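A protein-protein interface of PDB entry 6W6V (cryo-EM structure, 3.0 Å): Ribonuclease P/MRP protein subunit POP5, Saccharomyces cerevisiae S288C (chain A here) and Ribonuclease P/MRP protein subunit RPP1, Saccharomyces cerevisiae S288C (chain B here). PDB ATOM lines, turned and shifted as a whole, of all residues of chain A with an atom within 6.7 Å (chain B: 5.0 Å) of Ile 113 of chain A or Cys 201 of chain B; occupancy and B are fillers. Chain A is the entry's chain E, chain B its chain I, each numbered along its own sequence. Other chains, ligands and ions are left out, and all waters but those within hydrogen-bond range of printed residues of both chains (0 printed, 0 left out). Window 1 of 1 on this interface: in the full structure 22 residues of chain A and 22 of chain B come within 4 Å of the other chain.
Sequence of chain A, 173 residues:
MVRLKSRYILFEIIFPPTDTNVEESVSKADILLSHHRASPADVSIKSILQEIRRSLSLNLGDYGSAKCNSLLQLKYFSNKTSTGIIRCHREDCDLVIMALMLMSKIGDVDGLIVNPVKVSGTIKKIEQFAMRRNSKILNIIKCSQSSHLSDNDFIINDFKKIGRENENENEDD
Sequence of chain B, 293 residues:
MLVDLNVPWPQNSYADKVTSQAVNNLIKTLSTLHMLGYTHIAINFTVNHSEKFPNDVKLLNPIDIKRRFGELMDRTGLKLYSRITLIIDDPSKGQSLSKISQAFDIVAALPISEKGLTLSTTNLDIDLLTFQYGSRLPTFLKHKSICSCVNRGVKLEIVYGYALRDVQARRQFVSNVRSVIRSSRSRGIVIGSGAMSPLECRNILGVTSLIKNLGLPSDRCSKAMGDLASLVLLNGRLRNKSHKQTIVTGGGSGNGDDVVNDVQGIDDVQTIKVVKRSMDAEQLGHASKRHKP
The side-chain amide oxygen (OD1) of Asn 115 of chain A is in hydrogen-bond range of the side-chain amide nitrogen (ND2) of Asn 203 of chain B (3.2 Å).
The backbone NH of Glu 12 of chain A lies within hydrogen-bond range of the backbone carbonyl oxygen of Asn 115 of chain A, 2.9 Å away. NH1 of Arg 202 of chain B lies within hydrogen-bond range of O of Leu 199 of chain B (3.2 Å). N of Ile 14 of chain A is in hydrogen-bond range of O of Ile 113 of chain A (2.9 Å).
Among the printed residues, merely in contact across the chains: Asn 115 of chain A with Leu 36 of chain B (3.5 Å), Pro 16 of chain A with Leu 199 of chain B (3.6 Å), Ile 113 of chain A with Cys 201 of chain B (3.8 Å), Ile 113 of chain A with Leu 199 of chain B (3.8 Å) and Ile 14 of chain A with Leu 36 of chain B (3.9 Å).
Of the printed residues of chain B, Ile 113 of chain A touches Leu 199 and Cys 201. Of chain A, only Ile 113 comes within 4 Å of Cys 201 of chain B. Of the printed residues of chain A, Asn 203 of chain B touches Asn 115 (3.2 Å). Of the printed residues of chain B, Asn 115 of chain A touches Leu 36 and Asn 203. Of the printed residues of chain B, Ile 14 of chain A touches Leu 36 (3.9 Å). Of the printed residues of chain A, Leu 199 of chain B touches Pro 16 (3.6 Å) and Ile 113 (3.8 Å). Of the printed residues of chain B, Pro 16 of chain A touches Leu 199 (3.6 Å). The nearest residue of chain B that does not touch Ile 113 of chain A is Arg 202 of chain B (4.2 Å). The nearest printed residue of chain B that does not touch Asn 115 of chain A is Arg 202 of chain B (5.2 Å).
Printed residues of chain A that touch a printed residue of chain B: Ile 14, Pro 16, Ile 113 and Asn 115. Hydrophobic or aromatic side chains of chain A that line the printed part of chain B: Ile 14, Pro 16 and Ile 113. Among the printed residues, 6 pairs touch across the chains. Among the printed residues, no Asp or Glu carboxylate lies within 4 Å of a Lys or Arg side-chain nitrogen of the other chain.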
ATOM      1  N   GLU A  12      16.932  19.691 -23.791  1.00  0.00           N
ATOM      2  CA  GLU A  12      16.239  20.352 -22.696  1.00  0.00           C
ATOM      3  C   GLU A  12      16.538  19.635 -21.388  1.00  0.00           C
ATOM      4  O   GLU A  12      17.104  18.541 -21.363  1.00  0.00           O
ATOM      5  CB  GLU A  12      14.728  20.377 -22.942  1.00  0.00           C
ATOM      6  CG  GLU A  12      14.332  20.869 -24.313  1.00  0.00           C
ATOM      7  CD  GLU A  12      12.926  21.428 -24.335  1.00  0.00           C
ATOM      8  OE1 GLU A  12      12.169  21.157 -23.380  1.00  0.00           O
ATOM      9  OE2 GLU A  12      12.578  22.138 -25.301  1.00  0.00           O
ATOM     10  N   ILE A  13      16.144  20.261 -20.285  1.00  0.00           N
ATOM     11  CA  ILE A  13      16.294  19.674 -18.960  1.00  0.00           C
ATOM     12  C   ILE A  13      14.949  19.743 -18.256  1.00  0.00           C
ATOM     13  O   ILE A  13      14.416  20.837 -18.037  1.00  0.00           O
ATOM     14  CB  ILE A  13      17.376  20.382 -18.132  1.00  0.00           C
ATOM     15  CG1 ILE A  13      18.748  20.168 -18.762  1.00  0.00           C
ATOM     16  CG2 ILE A  13      17.377  19.865 -16.719  1.00  0.00           C
ATOM     17  CD1 ILE A  13      19.880  20.722 -17.942  1.00  0.00           C
ATOM     18  N   ILE A  14      14.407  18.585 -17.895  1.00  0.00           N
ATOM     19  CA  ILE A  14      13.128  18.493 -17.203  1.00  0.00           C
ATOM     20  C   ILE A  14      13.388  18.228 -15.728  1.00  0.00           C
ATOM     21  O   ILE A  14      14.208  17.370 -15.377  1.00  0.00           O
ATOM     22  CB  ILE A  14      12.240  17.397 -17.813  1.00  0.00           C
ATOM     23  CG1 ILE A  14      11.885  17.742 -19.257  1.00  0.00           C
ATOM     24  CG2 ILE A  14      10.983  17.203 -16.994  1.00  0.00           C
ATOM     25  CD1 ILE A  14      11.223  16.612 -20.003  1.00  0.00           C
ATOM     26  N   PHE A  15      12.692  18.966 -14.865  1.00  0.00           N
ATOM     27  CA  PHE A  15      12.827  18.853 -13.421  1.00  0.00           C
ATOM     28  C   PHE A  15      11.550  18.283 -12.812  1.00  0.00           C
ATOM     29  O   PHE A  15      10.728  19.042 -12.287  1.00  0.00           O
ATOM     30  CB  PHE A  15      13.126  20.222 -12.815  1.00  0.00           C
ATOM     31  CG  PHE A  15      14.584  20.558 -12.758  1.00  0.00           C
ATOM     32  CD1 PHE A  15      15.428  19.876 -11.906  1.00  0.00           C
ATOM     33  CD2 PHE A  15      15.107  21.573 -13.539  1.00  0.00           C
ATOM     34  CE1 PHE A  15      16.771  20.188 -11.847  1.00  0.00           C
ATOM     35  CE2 PHE A  15      16.450  21.893 -13.481  1.00  0.00           C
ATOM     36  CZ  PHE A  15      17.282  21.197 -12.635  1.00  0.00           C
ATOM     37  N   PRO A  16      11.349  16.965 -12.850  1.00  0.00           N
ATOM     38  CA  PRO A  16      10.084  16.409 -12.379  1.00  0.00           C
ATOM     39  C   PRO A  16       9.945  16.564 -10.877  1.00  0.00           C
ATOM     40  O   PRO A  16      10.950  16.641 -10.149  1.00  0.00           O
ATOM     41  CB  PRO A  16      10.175  14.928 -12.785  1.00  0.00           C
ATOM     42  CG  PRO A  16      11.615  14.653 -12.845  1.00  0.00           C
ATOM     43  CD  PRO A  16      12.279  15.917 -13.298  1.00  0.00           C
ATOM     44  N   LEU A 100      24.041  11.176 -22.979  1.00  0.00           N
ATOM     45  CA  LEU A 100      22.948  12.001 -22.475  1.00  0.00           C
ATOM     46  C   LEU A 100      22.023  11.205 -21.561  1.00  0.00           C
ATOM     47  O   LEU A 100      21.745  11.621 -20.431  1.00  0.00           O
ATOM     48  CB  LEU A 100      22.160  12.605 -23.636  1.00  0.00           C
ATOM     49  CG  LEU A 100      22.805  13.762 -24.401  1.00  0.00           C
ATOM     50  CD1 LEU A 100      21.880  14.221 -25.511  1.00  0.00           C
ATOM     51  CD2 LEU A 100      23.139  14.907 -23.468  1.00  0.00           C
ATOM     52  N   MET A 103      23.257   9.700 -18.061  1.00  0.00           N
ATOM     53  CA  MET A 103      23.764  10.734 -17.169  1.00  0.00           C
ATOM     54  C   MET A 103      22.599  11.426 -16.481  1.00  0.00           C
ATOM     55  O   MET A 103      21.693  11.937 -17.146  1.00  0.00           O
ATOM     56  CB  MET A 103      24.600  11.761 -17.932  1.00  0.00           C
ATOM     57  CG  MET A 103      25.080  12.913 -17.078  1.00  0.00           C
ATOM     58  SD  MET A 103      25.901  14.187 -18.045  1.00  0.00           S
ATOM     59  CE  MET A 103      24.493  15.129 -18.616  1.00  0.00           C
ATOM     60  N   SER A 104      22.628  11.441 -15.154  1.00  0.00           N
ATOM     61  CA  SER A 104      21.718  12.227 -14.336  1.00  0.00           C
ATOM     62  C   SER A 104      22.531  12.869 -13.222  1.00  0.00           C
ATOM     63  O   SER A 104      23.726  12.603 -13.073  1.00  0.00           O
ATOM     64  CB  SER A 104      20.586  11.362 -13.773  1.00  0.00           C
ATOM     65  OG  SER A 104      21.105  10.232 -13.097  1.00  0.00           O
ATOM     66  N   ILE A 106      23.377  16.262 -12.543  1.00  0.00           N
ATOM     67  CA  ILE A 106      24.378  17.173 -13.089  1.00  0.00           C
ATOM     68  C   ILE A 106      25.072  17.902 -11.946  1.00  0.00           C
ATOM     69  O   ILE A 106      24.425  18.584 -11.144  1.00  0.00           O
ATOM     70  CB  ILE A 106      23.740  18.167 -14.066  1.00  0.00           C
ATOM     71  CG1 ILE A 106      23.331  17.460 -15.354  1.00  0.00           C
ATOM     72  CG2 ILE A 106      24.693  19.308 -14.356  1.00  0.00           C
ATOM     73  CD1 ILE A 106      22.367  18.250 -16.199  1.00  0.00           C
ATOM     74  N   GLY A 111      17.945  14.725  -9.294  1.00  0.00           N
ATOM     75  CA  GLY A 111      16.562  14.522  -9.673  1.00  0.00           C
ATOM     76  C   GLY A 111      16.139  15.301 -10.899  1.00  0.00           C
ATOM     77  O   GLY A 111      15.336  16.231 -10.799  1.00  0.00           O
ATOM     78  N   LEU A 112      16.676  14.937 -12.060  1.00  0.00           N
ATOM     79  CA  LEU A 112      16.387  15.653 -13.294  1.00  0.00           C
ATOM     80  C   LEU A 112      16.596  14.717 -14.474  1.00  0.00           C
ATOM     81  O   LEU A 112      17.195  13.646 -14.347  1.00  0.00           O
ATOM     82  CB  LEU A 112      17.258  16.904 -13.437  1.00  0.00           C
ATOM     83  CG  LEU A 112      18.737  16.717 -13.766  1.00  0.00           C
ATOM     84  CD1 LEU A 112      19.316  18.025 -14.236  1.00  0.00           C
ATOM     85  CD2 LEU A 112      19.507  16.223 -12.560  1.00  0.00           C
ATOM     86  N   ILE A 113      16.088  15.130 -15.631  1.00  0.00           N
ATOM     87  CA  ILE A 113      16.191  14.352 -16.859  1.00  0.00           C
ATOM     88  C   ILE A 113      16.746  15.247 -17.956  1.00  0.00           C
ATOM     89  O   ILE A 113      16.283  16.379 -18.130  1.00  0.00           O
ATOM     90  CB  ILE A 113      14.829  13.771 -17.279  1.00  0.00           C
ATOM     91  CG1 ILE A 113      14.343  12.759 -16.247  1.00  0.00           C
ATOM     92  CG2 ILE A 113      14.926  13.121 -18.638  1.00  0.00           C
ATOM     93  CD1 ILE A 113      13.085  12.041 -16.660  1.00  0.00           C
ATOM     94  N   VAL A 114      17.735  14.746 -18.691  1.00  0.00           N
ATOM     95  CA  VAL A 114      18.287  15.439 -19.849  1.00  0.00           C
ATOM     96  C   VAL A 114      17.648  14.844 -21.096  1.00  0.00           C
ATOM     97  O   VAL A 114      17.735  13.634 -21.330  1.00  0.00           O
ATOM     98  CB  VAL A 114      19.815  15.324 -19.897  1.00  0.00           C
ATOM     99  CG1 VAL A 114      20.369  16.209 -20.989  1.00  0.00           C
ATOM    100  CG2 VAL A 114      20.406  15.706 -18.557  1.00  0.00           C
ATOM    101  N   ASN A 115      17.011  15.690 -21.900  1.00  0.00           N
ATOM    102  CA  ASN A 115      16.104  15.241 -22.953  1.00  0.00           C
ATOM    103  C   ASN A 115      16.530  15.806 -24.300  1.00  0.00           C
ATOM    104  O   ASN A 115      16.293  16.994 -24.577  1.00  0.00           O
ATOM    105  CB  ASN A 115      14.681  15.668 -22.623  1.00  0.00           C
ATOM    106  CG  ASN A 115      13.650  14.704 -23.138  1.00  0.00           C
ATOM    107  OD1 ASN A 115      13.889  13.501 -23.201  1.00  0.00           O
ATOM    108  ND2 ASN A 115      12.489  15.224 -23.511  1.00  0.00           N
ATOM    109  N   LEU B  33       5.375  10.205 -18.181  1.00  0.00           N
ATOM    110  CA  LEU B  33       5.428   9.436 -19.420  1.00  0.00           C
ATOM    111  C   LEU B  33       4.527  10.033 -20.490  1.00  0.00           C
ATOM    112  O   LEU B  33       4.873  10.004 -21.674  1.00  0.00           O
ATOM    113  CB  LEU B  33       5.051   7.976 -19.173  1.00  0.00           C
ATOM    114  CG  LEU B  33       6.179   6.997 -18.848  1.00  0.00           C
ATOM    115  CD1 LEU B  33       6.755   7.237 -17.471  1.00  0.00           C
ATOM    116  CD2 LEU B  33       5.682   5.572 -18.972  1.00  0.00           C
ATOM    117  N   LEU B  36       6.484  12.947 -22.022  1.00  0.00           N
ATOM    118  CA  LEU B  36       7.619  12.627 -22.883  1.00  0.00           C
ATOM    119  C   LEU B  36       7.201  12.200 -24.283  1.00  0.00           C
ATOM    120  O   LEU B  36       8.029  12.238 -25.196  1.00  0.00           O
ATOM    121  CB  LEU B  36       8.489  11.546 -22.252  1.00  0.00           C
ATOM    122  CG  LEU B  36       9.438  12.093 -21.191  1.00  0.00           C
ATOM    123  CD1 LEU B  36      10.344  11.009 -20.666  1.00  0.00           C
ATOM    124  CD2 LEU B  36      10.251  13.229 -21.764  1.00  0.00           C
ATOM    125  N   TYR B  38       4.723   9.361 -24.976  1.00  0.00           N
ATOM    126  CA  TYR B  38       3.972   8.116 -25.039  1.00  0.00           C
ATOM    127  C   TYR B  38       2.476   8.380 -24.954  1.00  0.00           C
ATOM    128  O   TYR B  38       2.024   9.253 -24.212  1.00  0.00           O
ATOM    129  CB  TYR B  38       4.399   7.181 -23.914  1.00  0.00           C
ATOM    130  CG  TYR B  38       5.841   6.757 -23.995  1.00  0.00           C
ATOM    131  CD1 TYR B  38       6.212   5.642 -24.723  1.00  0.00           C
ATOM    132  CD2 TYR B  38       6.829   7.471 -23.347  1.00  0.00           C
ATOM    133  CE1 TYR B  38       7.527   5.250 -24.801  1.00  0.00           C
ATOM    134  CE2 TYR B  38       8.147   7.087 -23.419  1.00  0.00           C
ATOM    135  CZ  TYR B  38       8.489   5.977 -24.147  1.00  0.00           C
ATOM    136  OH  TYR B  38       9.803   5.589 -24.223  1.00  0.00           O
ATOM    137  N   TYR B 160      15.117  -2.176 -20.511  1.00  0.00           N
ATOM    138  CA  TYR B 160      16.092  -1.089 -20.402  1.00  0.00           C
ATOM    139  C   TYR B 160      15.986  -0.349 -19.074  1.00  0.00           C
ATOM    140  O   TYR B 160      16.734   0.602 -18.832  1.00  0.00           O
ATOM    141  CB  TYR B 160      16.005  -0.097 -21.578  1.00  0.00           C
ATOM    142  CG  TYR B 160      14.931   0.979 -21.541  1.00  0.00           C
ATOM    143  CD1 TYR B 160      13.757   0.848 -22.267  1.00  0.00           C
ATOM    144  CD2 TYR B 160      15.119   2.151 -20.819  1.00  0.00           C
ATOM    145  CE1 TYR B 160      12.790   1.833 -22.244  1.00  0.00           C
ATOM    146  CE2 TYR B 160      14.156   3.137 -20.789  1.00  0.00           C
ATOM    147  CZ  TYR B 160      12.996   2.973 -21.505  1.00  0.00           C
ATOM    148  OH  TYR B 160      12.035   3.954 -21.480  1.00  0.00           O
ATOM    149  N   LEU B 164      19.381   1.824 -15.734  1.00  0.00           N
ATOM    150  CA  LEU B 164      19.292   3.141 -15.126  1.00  0.00           C
ATOM    151  C   LEU B 164      19.445   3.123 -13.614  1.00  0.00           C
ATOM    152  O   LEU B 164      19.665   4.183 -13.020  1.00  0.00           O
ATOM    153  CB  LEU B 164      17.949   3.788 -15.486  1.00  0.00           C
ATOM    154  CG  LEU B 164      17.751   4.063 -16.973  1.00  0.00           C
ATOM    155  CD1 LEU B 164      16.328   4.490 -17.249  1.00  0.00           C
ATOM    156  CD2 LEU B 164      18.724   5.123 -17.432  1.00  0.00           C
ATOM    157  N   ALA B 195       9.464   1.384 -15.087  1.00  0.00           N
ATOM    158  CA  ALA B 195       9.518   2.706 -14.475  1.00  0.00           C
ATOM    159  C   ALA B 195       8.971   2.606 -13.056  1.00  0.00           C
ATOM    160  O   ALA B 195       7.767   2.725 -12.828  1.00  0.00           O
ATOM    161  CB  ALA B 195       8.738   3.716 -15.304  1.00  0.00           C
ATOM    162  N   SER B 197       9.673   4.783 -10.829  1.00  0.00           N
ATOM    163  CA  SER B 197       9.742   6.140 -10.310  1.00  0.00           C
ATOM    164  C   SER B 197       9.497   7.098 -11.465  1.00  0.00           C
ATOM    165  O   SER B 197       9.669   6.723 -12.629  1.00  0.00           O
ATOM    166  CB  SER B 197      11.109   6.407  -9.658  1.00  0.00           C
ATOM    167  OG  SER B 197      11.214   7.726  -9.159  1.00  0.00           O
ATOM    168  N   PRO B 198       9.085   8.334 -11.185  1.00  0.00           N
ATOM    169  CA  PRO B 198       8.942   9.314 -12.269  1.00  0.00           C
ATOM    170  C   PRO B 198      10.278   9.867 -12.738  1.00  0.00           C
ATOM    171  O   PRO B 198      10.328  10.880 -13.439  1.00  0.00           O
ATOM    172  CB  PRO B 198       8.066  10.406 -11.644  1.00  0.00           C
ATOM    173  CG  PRO B 198       8.284  10.276 -10.192  1.00  0.00           C
ATOM    174  CD  PRO B 198       8.486   8.817  -9.931  1.00  0.00           C
ATOM    175  N   LEU B 199      11.369   9.216 -12.346  1.00  0.00           N
ATOM    176  CA  LEU B 199      12.699   9.583 -12.803  1.00  0.00           C
ATOM    177  C   LEU B 199      13.287   8.603 -13.801  1.00  0.00           C
ATOM    178  O   LEU B 199      14.137   8.992 -14.602  1.00  0.00           O
ATOM    179  CB  LEU B 199      13.655   9.692 -11.611  1.00  0.00           C
ATOM    180  CG  LEU B 199      13.154  10.551 -10.456  1.00  0.00           C
ATOM    181  CD1 LEU B 199      14.127  10.506  -9.292  1.00  0.00           C
ATOM    182  CD2 LEU B 199      12.936  11.968 -10.924  1.00  0.00           C
ATOM    183  N   GLU B 200      12.849   7.347 -13.778  1.00  0.00           N
ATOM    184  CA  GLU B 200      13.463   6.289 -14.564  1.00  0.00           C
ATOM    185  C   GLU B 200      12.832   6.130 -15.939  1.00  0.00           C
ATOM    186  O   GLU B 200      12.887   5.036 -16.510  1.00  0.00           O
ATOM    187  CB  GLU B 200      13.394   4.967 -13.798  1.00  0.00           C
ATOM    188  CG  GLU B 200      14.018   5.038 -12.417  1.00  0.00           C
ATOM    189  CD  GLU B 200      14.698   3.748 -12.012  1.00  0.00           C
ATOM    190  OE1 GLU B 200      15.319   3.712 -10.929  1.00  0.00           O
ATOM    191  OE2 GLU B 200      14.610   2.767 -12.775  1.00  0.00           O
ATOM    192  N   CYS B 201      12.233   7.184 -16.481  1.00  0.00           N
ATOM    193  CA  CYS B 201      11.677   7.149 -17.824  1.00  0.00           C
ATOM    194  C   CYS B 201      12.570   7.925 -18.784  1.00  0.00           C
ATOM    195  O   CYS B 201      13.425   8.712 -18.374  1.00  0.00           O
ATOM    196  CB  CYS B 201      10.259   7.718 -17.841  1.00  0.00           C
ATOM    197  SG  CYS B 201       9.567   7.836 -19.496  1.00  0.00           S
ATOM    198  N   ARG B 202      12.353   7.705 -20.080  1.00  0.00           N
ATOM    199  CA  ARG B 202      13.217   8.283 -21.099  1.00  0.00           C
ATOM    200  C   ARG B 202      12.414   8.565 -22.360  1.00  0.00           C
ATOM    201  O   ARG B 202      11.277   8.117 -22.516  1.00  0.00           O
ATOM    202  CB  ARG B 202      14.395   7.361 -21.417  1.00  0.00           C
ATOM    203  CG  ARG B 202      15.560   7.477 -20.457  1.00  0.00           C
ATOM    204  CD  ARG B 202      15.924   8.924 -20.195  1.00  0.00           C
ATOM    205  NE  ARG B 202      16.959   9.042 -19.174  1.00  0.00           N
ATOM    206  CZ  ARG B 202      16.743   8.914 -17.870  1.00  0.00           C
ATOM    207  NH1 ARG B 202      15.523   8.666 -17.421  1.00  0.00           N
ATOM    208  NH2 ARG B 202      17.747   9.033 -17.017  1.00  0.00           N
ATOM    209  N   ASN B 203      13.037   9.310 -23.268  1.00  0.00           N
ATOM    210  CA  ASN B 203      12.431   9.696 -24.535  1.00  0.00           C
ATOM    211  C   ASN B 203      12.511   8.524 -25.510  1.00  0.00           C
ATOM    212  O   ASN B 203      12.812   7.391 -25.128  1.00  0.00           O
ATOM    213  CB  ASN B 203      13.120  10.940 -25.081  1.00  0.00           C
ATOM    214  CG  ASN B 203      12.244  11.714 -26.029  1.00  0.00           C
ATOM    215  OD1 ASN B 203      11.466  11.132 -26.782  1.00  0.00           O
ATOM    216  ND2 ASN B 203      12.363  13.034 -26.002  1.00  0.00           N
